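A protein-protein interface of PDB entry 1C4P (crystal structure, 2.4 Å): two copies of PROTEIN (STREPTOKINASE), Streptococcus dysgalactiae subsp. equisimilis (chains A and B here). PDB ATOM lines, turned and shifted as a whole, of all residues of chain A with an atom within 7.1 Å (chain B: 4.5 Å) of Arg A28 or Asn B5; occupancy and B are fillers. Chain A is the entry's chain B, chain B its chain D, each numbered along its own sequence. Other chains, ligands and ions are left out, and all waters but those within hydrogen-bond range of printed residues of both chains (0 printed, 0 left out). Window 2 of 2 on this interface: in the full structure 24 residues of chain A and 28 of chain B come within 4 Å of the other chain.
Glu B101 touches Pro A29. CE1 of Tyr B104 touches O of Pro A29, at 3.5 Å. Gly A30 touches Gln B102 (CA to O, 3.4 Å). CB of Leu A31 touches OH of Tyr B104 (3.1 Å).
N of Gln B4 is in hydrogen-bond range of OE1 of Glu B101, 3.3 Å away. OE2 of Glu B101 sits at hydrogen-bond distance from N of Asn B5. The backbone NH of Gln B102 sits at hydrogen-bond distance from the backbone carbonyl oxygen of Asn B5.
Printed residues of chain B that touch a printed residue of chain A: Asn B5, Glu B101, Gln B102, Tyr B104 and Glu B115. Hydrophobic or aromatic side chains of chain B within 4 Å of the printed part of chain A: Tyr B104. Of the 10 printed residues of chain A, 5 touch a printed residue of chain B. Among the printed residues, 10 pairs touch across the chains. Among the printed residues, Asp or Glu carboxylates within 4 Å of a Lys or Arg side-chain nitrogen of the other chain: Arg A28 with Glu B115.
Of chain B, only Asn B5, Tyr B104 and Glu B115 come within 4 Å of Arg A28. Of the printed residues of chain B, Pro A29 touches Glu B101 (3.2 Å), Gln B102 (3.3 Å) and Tyr B104 (3.5 Å). Printed residues of chain B within 4 Å of Leu A31: Tyr B104. Printed residues of chain B within 4 Å of Lys A32: Tyr B104 (2.7 Å). His A63 touches none of the printed residues of chain B. Gln B4 touches none of the printed residues of chain A. Asn B5 touches just one residue of chain A: Arg A28. The nearest residue of chain A that does not touch Asn B5 is Pro A29 (6.3 Å). The nearest printed residue of chain A that does not touch Glu B101 is Gly A30 (4.7 Å).
The guanidinium group of Arg A28 sits close to the side-chain amide nitrogen of Asn B5 (3.0 Å). The backbone carbonyl oxygen of Arg A28 sits at hydrogen-bond distance from the side-chain hydroxyl of Tyr B104 (2.6 Å). The guanidinium group (NH2) of Arg A28 lies within salt-bridge range of the side-chain carboxylate (OE2) of Glu B115. O of Gly A30 sits at hydrogen-bond distance from N of Tyr B104, 2.9 Å away. The backbone NH (N) of Lys A32 sits at hydrogen-bond distance from the backbone carbonyl oxygen (O) of Tyr B104, 2.7 Å away. The backbone carbonyl oxygen of Pro A29 sits close to the backbone carbonyl oxygen of Gln B102, at 3.3 Å.
No position is printed for both chains. Of the 10 pairs that touch across the chains among the printed residues, none has its exchanged pair printed and touching as well.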
ATOM      1  N   ASP A  24     -23.221  13.708  29.292  1.00  0.00           N
ATOM      2  CA  ASP A  24     -22.707  12.614  28.469  1.00  0.00           C
ATOM      3  C   ASP A  24     -22.223  13.096  27.096  1.00  0.00           C
ATOM      4  O   ASP A  24     -22.933  13.829  26.382  1.00  0.00           O
ATOM      5  CB  ASP A  24     -23.771  11.518  28.295  1.00  0.00           C
ATOM      6  CG  ASP A  24     -23.371  10.461  27.256  1.00  0.00           C
ATOM      7  OD1 ASP A  24     -23.293  10.806  26.055  1.00  0.00           O
ATOM      8  OD2 ASP A  24     -23.137   9.288  27.633  1.00  0.00           O
ATOM      9  N   ASP A  25     -21.007  12.667  26.750  1.00  0.00           N
ATOM     10  CA  ASP A  25     -20.350  13.012  25.492  1.00  0.00           C
ATOM     11  C   ASP A  25     -20.984  12.347  24.268  1.00  0.00           C
ATOM     12  O   ASP A  25     -21.139  12.985  23.225  1.00  0.00           O
ATOM     13  CB  ASP A  25     -18.858  12.650  25.573  1.00  0.00           C
ATOM     14  CG  ASP A  25     -18.225  12.442  24.203  1.00  0.00           C
ATOM     15  OD1 ASP A  25     -18.536  11.421  23.547  1.00  0.00           O
ATOM     16  OD2 ASP A  25     -17.419  13.299  23.780  1.00  0.00           O
ATOM     17  N   ASP A  26     -21.343  11.070  24.392  1.00  0.00           N
ATOM     18  CA  ASP A  26     -21.955  10.330  23.289  1.00  0.00           C
ATOM     19  C   ASP A  26     -23.071  11.125  22.620  1.00  0.00           C
ATOM     20  O   ASP A  26     -23.346  10.946  21.428  1.00  0.00           O
ATOM     21  CB  ASP A  26     -22.509   8.983  23.786  1.00  0.00           C
ATOM     22  CG  ASP A  26     -21.678   7.785  23.307  1.00  0.00           C
ATOM     23  OD1 ASP A  26     -21.560   7.588  22.075  1.00  0.00           O
ATOM     24  OD2 ASP A  26     -21.148   7.039  24.164  1.00  0.00           O
ATOM     25  N   PHE A  27     -23.711  12.001  23.391  1.00  0.00           N
ATOM     26  CA  PHE A  27     -24.794  12.819  22.867  1.00  0.00           C
ATOM     27  C   PHE A  27     -24.268  14.013  22.119  1.00  0.00           C
ATOM     28  O   PHE A  27     -24.283  15.149  22.612  1.00  0.00           O
ATOM     29  CB  PHE A  27     -25.735  13.254  23.987  1.00  0.00           C
ATOM     30  CG  PHE A  27     -26.584  12.141  24.500  1.00  0.00           C
ATOM     31  CD1 PHE A  27     -26.042  11.166  25.329  1.00  0.00           C
ATOM     32  CD2 PHE A  27     -27.909  12.020  24.096  1.00  0.00           C
ATOM     33  CE1 PHE A  27     -26.801  10.083  25.749  1.00  0.00           C
ATOM     34  CE2 PHE A  27     -28.678  10.946  24.506  1.00  0.00           C
ATOM     35  CZ  PHE A  27     -28.121   9.968  25.339  1.00  0.00           C
ATOM     36  N   ARG A  28     -23.793  13.708  20.915  1.00  0.00           N
ATOM     37  CA  ARG A  28     -23.230  14.668  19.980  1.00  0.00           C
ATOM     38  C   ARG A  28     -24.360  15.597  19.509  1.00  0.00           C
ATOM     39  O   ARG A  28     -25.353  15.150  18.931  1.00  0.00           O
ATOM     40  CB  ARG A  28     -22.613  13.902  18.786  1.00  0.00           C
ATOM     41  CG  ARG A  28     -21.642  14.685  17.877  1.00  0.00           C
ATOM     42  CD  ARG A  28     -21.063  13.773  16.774  1.00  0.00           C
ATOM     43  NE  ARG A  28     -19.971  14.367  15.981  1.00  0.00           N
ATOM     44  CZ  ARG A  28     -20.120  15.107  14.874  1.00  0.00           C
ATOM     45  NH1 ARG A  28     -21.325  15.381  14.386  1.00  0.00           N
ATOM     46  NH2 ARG A  28     -19.051  15.551  14.222  1.00  0.00           N
ATOM     47  N   PRO A  29     -24.234  16.905  19.782  1.00  0.00           N
ATOM     48  CA  PRO A  29     -25.246  17.881  19.374  1.00  0.00           C
ATOM     49  C   PRO A  29     -25.232  18.091  17.852  1.00  0.00           C
ATOM     50  O   PRO A  29     -24.197  17.894  17.187  1.00  0.00           O
ATOM     51  CB  PRO A  29     -24.833  19.133  20.140  1.00  0.00           C
ATOM     52  CG  PRO A  29     -23.339  19.014  20.179  1.00  0.00           C
ATOM     53  CD  PRO A  29     -23.156  17.558  20.548  1.00  0.00           C
ATOM     54  N   GLY A  30     -26.381  18.483  17.303  1.00  0.00           N
ATOM     55  CA  GLY A  30     -26.470  18.707  15.875  1.00  0.00           C
ATOM     56  C   GLY A  30     -27.037  17.519  15.120  1.00  0.00           C
ATOM     57  O   GLY A  30     -27.031  17.507  13.886  1.00  0.00           O
ATOM     58  N   LEU A  31     -27.528  16.519  15.846  1.00  0.00           N
ATOM     59  CA  LEU A  31     -28.094  15.337  15.196  1.00  0.00           C
ATOM     60  C   LEU A  31     -29.395  15.670  14.469  1.00  0.00           C
ATOM     61  O   LEU A  31     -30.261  16.354  15.002  1.00  0.00           O
ATOM     62  CB  LEU A  31     -28.336  14.221  16.216  1.00  0.00           C
ATOM     63  CG  LEU A  31     -29.083  12.989  15.691  1.00  0.00           C
ATOM     64  CD1 LEU A  31     -28.401  12.484  14.424  1.00  0.00           C
ATOM     65  CD2 LEU A  31     -29.151  11.905  16.779  1.00  0.00           C
ATOM     66  N   LYS A  32     -29.505  15.179  13.244  1.00  0.00           N
ATOM     67  CA  LYS A  32     -30.663  15.408  12.402  1.00  0.00           C
ATOM     68  C   LYS A  32     -31.247  14.065  12.005  1.00  0.00           C
ATOM     69  O   LYS A  32     -30.627  13.303  11.266  1.00  0.00           O
ATOM     70  CB  LYS A  32     -30.240  16.181  11.156  1.00  0.00           C
ATOM     71  CG  LYS A  32     -31.301  16.312  10.086  1.00  0.00           C
ATOM     72  CD  LYS A  32     -30.782  17.227   8.991  1.00  0.00           C
ATOM     73  CE  LYS A  32     -31.732  17.359   7.814  1.00  0.00           C
ATOM     74  NZ  LYS A  32     -31.065  18.130   6.707  1.00  0.00           N
ATOM     75  N   HIS A  63     -29.311   5.500  21.128  1.00  0.00           N
ATOM     76  CA  HIS A  63     -28.696   5.616  22.463  1.00  0.00           C
ATOM     77  C   HIS A  63     -29.203   4.533  23.407  1.00  0.00           C
ATOM     78  O   HIS A  63     -29.722   4.839  24.494  1.00  0.00           O
ATOM     79  CB  HIS A  63     -29.007   6.967  23.111  1.00  0.00           C
ATOM     80  CG  HIS A  63     -28.446   8.136  22.376  1.00  0.00           C
ATOM     81  ND1 HIS A  63     -27.173   8.615  22.600  1.00  0.00           N
ATOM     82  CD2 HIS A  63     -28.964   8.891  21.379  1.00  0.00           C
ATOM     83  CE1 HIS A  63     -26.930   9.610  21.768  1.00  0.00           C
ATOM     84  NE2 HIS A  63     -27.998   9.798  21.016  1.00  0.00           N
ATOM     85  N   ILE B   3     -19.723  26.131  21.675  1.00  0.00           N
ATOM     86  CA  ILE B   3     -19.504  25.575  20.333  1.00  0.00           C
ATOM     87  C   ILE B   3     -18.249  24.730  20.138  1.00  0.00           C
ATOM     88  O   ILE B   3     -17.217  25.226  19.687  1.00  0.00           O
ATOM     89  CB  ILE B   3     -19.520  26.694  19.240  1.00  0.00           C
ATOM     90  CG1 ILE B   3     -19.082  28.043  19.840  1.00  0.00           C
ATOM     91  CG2 ILE B   3     -20.909  26.789  18.613  1.00  0.00           C
ATOM     92  CD1 ILE B   3     -17.582  28.191  20.077  1.00  0.00           C
ATOM     93  N   GLN B   4     -18.346  23.443  20.451  1.00  0.00           N
ATOM     94  CA  GLN B   4     -17.203  22.556  20.291  1.00  0.00           C
ATOM     95  C   GLN B   4     -16.897  22.264  18.830  1.00  0.00           C
ATOM     96  O   GLN B   4     -15.926  22.789  18.287  1.00  0.00           O
ATOM     97  CB  GLN B   4     -17.429  21.243  21.036  1.00  0.00           C
ATOM     98  CG  GLN B   4     -17.284  21.362  22.550  1.00  0.00           C
ATOM     99  CD  GLN B   4     -16.926  20.037  23.202  1.00  0.00           C
ATOM    100  OE1 GLN B   4     -15.849  19.482  22.955  1.00  0.00           O
ATOM    101  NE2 GLN B   4     -17.830  19.518  24.031  1.00  0.00           N
ATOM    102  N   ASN B   5     -17.714  21.424  18.199  1.00  0.00           N
ATOM    103  CA  ASN B   5     -17.517  21.081  16.792  1.00  0.00           C
ATOM    104  C   ASN B   5     -18.322  22.043  15.912  1.00  0.00           C
ATOM    105  O   ASN B   5     -19.470  21.780  15.572  1.00  0.00           O
ATOM    106  CB  ASN B   5     -17.972  19.644  16.527  1.00  0.00           C
ATOM    107  CG  ASN B   5     -17.366  19.058  15.259  1.00  0.00           C
ATOM    108  OD1 ASN B   5     -17.063  19.779  14.303  1.00  0.00           O
ATOM    109  ND2 ASN B   5     -17.194  17.739  15.245  1.00  0.00           N
ATOM    110  N   GLN B   6     -17.712  23.154  15.535  1.00  0.00           N
ATOM    111  CA  GLN B   6     -18.394  24.150  14.718  1.00  0.00           C
ATOM    112  C   GLN B   6     -18.798  23.687  13.301  1.00  0.00           C
ATOM    113  O   GLN B   6     -18.028  23.014  12.606  1.00  0.00           O
ATOM    114  CB  GLN B   6     -17.509  25.381  14.621  1.00  0.00           C
ATOM    115  CG  GLN B   6     -18.169  26.577  14.002  1.00  0.00           C
ATOM    116  CD  GLN B   6     -17.169  27.619  13.570  1.00  0.00           C
ATOM    117  OE1 GLN B   6     -16.544  27.492  12.513  1.00  0.00           O
ATOM    118  NE2 GLN B   6     -16.993  28.652  14.395  1.00  0.00           N
ATOM    119  N   ALA B   7     -20.009  24.057  12.874  1.00  0.00           N
ATOM    120  CA  ALA B   7     -20.487  23.693  11.544  1.00  0.00           C
ATOM    121  C   ALA B   7     -19.540  24.203  10.467  1.00  0.00           C
ATOM    122  O   ALA B   7     -18.995  25.292  10.573  1.00  0.00           O
ATOM    123  CB  ALA B   7     -21.863  24.252  11.300  1.00  0.00           C
ATOM    124  N   ARG B 100     -22.714  27.731  15.013  1.00  0.00           N
ATOM    125  CA  ARG B 100     -23.439  26.605  15.570  1.00  0.00           C
ATOM    126  C   ARG B 100     -22.669  25.283  15.489  1.00  0.00           C
ATOM    127  O   ARG B 100     -21.655  25.160  14.789  1.00  0.00           O
ATOM    128  CB  ARG B 100     -24.745  26.434  14.815  1.00  0.00           C
ATOM    129  CG  ARG B 100     -24.526  25.756  13.481  1.00  0.00           C
ATOM    130  CD  ARG B 100     -25.633  26.074  12.512  1.00  0.00           C
ATOM    131  NE  ARG B 100     -25.654  27.483  12.135  1.00  0.00           N
ATOM    132  CZ  ARG B 100     -26.595  28.004  11.366  1.00  0.00           C
ATOM    133  NH1 ARG B 100     -27.570  27.223  10.917  1.00  0.00           N
ATOM    134  NH2 ARG B 100     -26.562  29.287  11.032  1.00  0.00           N
ATOM    135  N   GLU B 101     -23.204  24.297  16.200  1.00  0.00           N
ATOM    136  CA  GLU B 101     -22.654  22.961  16.231  1.00  0.00           C
ATOM    137  C   GLU B 101     -22.919  22.246  14.894  1.00  0.00           C
ATOM    138  O   GLU B 101     -23.971  22.409  14.266  1.00  0.00           O
ATOM    139  CB  GLU B 101     -23.285  22.173  17.379  1.00  0.00           C
ATOM    140  CG  GLU B 101     -22.346  21.177  17.998  1.00  0.00           C
ATOM    141  CD  GLU B 101     -21.181  21.860  18.700  1.00  0.00           C
ATOM    142  OE1 GLU B 101     -21.366  22.311  19.862  1.00  0.00           O
ATOM    143  OE2 GLU B 101     -20.088  21.956  18.078  1.00  0.00           O
ATOM    144  N   GLN B 102     -21.941  21.456  14.474  1.00  0.00           N
ATOM    145  CA  GLN B 102     -21.993  20.698  13.245  1.00  0.00           C
ATOM    146  C   GLN B 102     -23.193  19.763  13.198  1.00  0.00           C
ATOM    147  O   GLN B 102     -23.515  19.075  14.167  1.00  0.00           O
ATOM    148  CB  GLN B 102     -20.697  19.899  13.097  1.00  0.00           C
ATOM    149  CG  GLN B 102     -20.652  19.028  11.878  1.00  0.00           C
ATOM    150  CD  GLN B 102     -20.754  19.821  10.603  1.00  0.00           C
ATOM    151  OE1 GLN B 102     -19.963  20.734  10.376  1.00  0.00           O
ATOM    152  NE2 GLN B 102     -21.719  19.479   9.756  1.00  0.00           N
ATOM    153  N   TYR B 104     -25.232  16.486  11.828  1.00  0.00           N
ATOM    154  CA  TYR B 104     -24.922  15.149  11.381  1.00  0.00           C
ATOM    155  C   TYR B 104     -26.200  14.308  11.414  1.00  0.00           C
ATOM    156  O   TYR B 104     -27.212  14.735  11.973  1.00  0.00           O
ATOM    157  CB  TYR B 104     -23.826  14.537  12.271  1.00  0.00           C
ATOM    158  CG  TYR B 104     -24.292  14.138  13.647  1.00  0.00           C
ATOM    159  CD1 TYR B 104     -24.344  15.070  14.686  1.00  0.00           C
ATOM    160  CD2 TYR B 104     -24.712  12.836  13.909  1.00  0.00           C
ATOM    161  CE1 TYR B 104     -24.807  14.714  15.958  1.00  0.00           C
ATOM    162  CE2 TYR B 104     -25.178  12.467  15.171  1.00  0.00           C
ATOM    163  CZ  TYR B 104     -25.226  13.410  16.191  1.00  0.00           C
ATOM    164  OH  TYR B 104     -25.717  13.051  17.430  1.00  0.00           O
ATOM    165  N   GLU B 115     -21.290  13.685   8.752  1.00  0.00           N
ATOM    166  CA  GLU B 115     -21.496  15.111   8.785  1.00  0.00           C
ATOM    167  C   GLU B 115     -22.299  15.552   7.584  1.00  0.00           C
ATOM    168  O   GLU B 115     -22.076  15.090   6.478  1.00  0.00           O
ATOM    169  CB  GLU B 115     -20.168  15.853   8.766  1.00  0.00           C
ATOM    170  CG  GLU B 115     -19.310  15.613   9.978  1.00  0.00           C
ATOM    171  CD  GLU B 115     -18.174  16.604  10.054  1.00  0.00           C
ATOM    172  OE1 GLU B 115     -17.837  17.188   8.996  1.00  0.00           O
ATOM    173  OE2 GLU B 115     -17.628  16.793  11.165  1.00  0.00           O
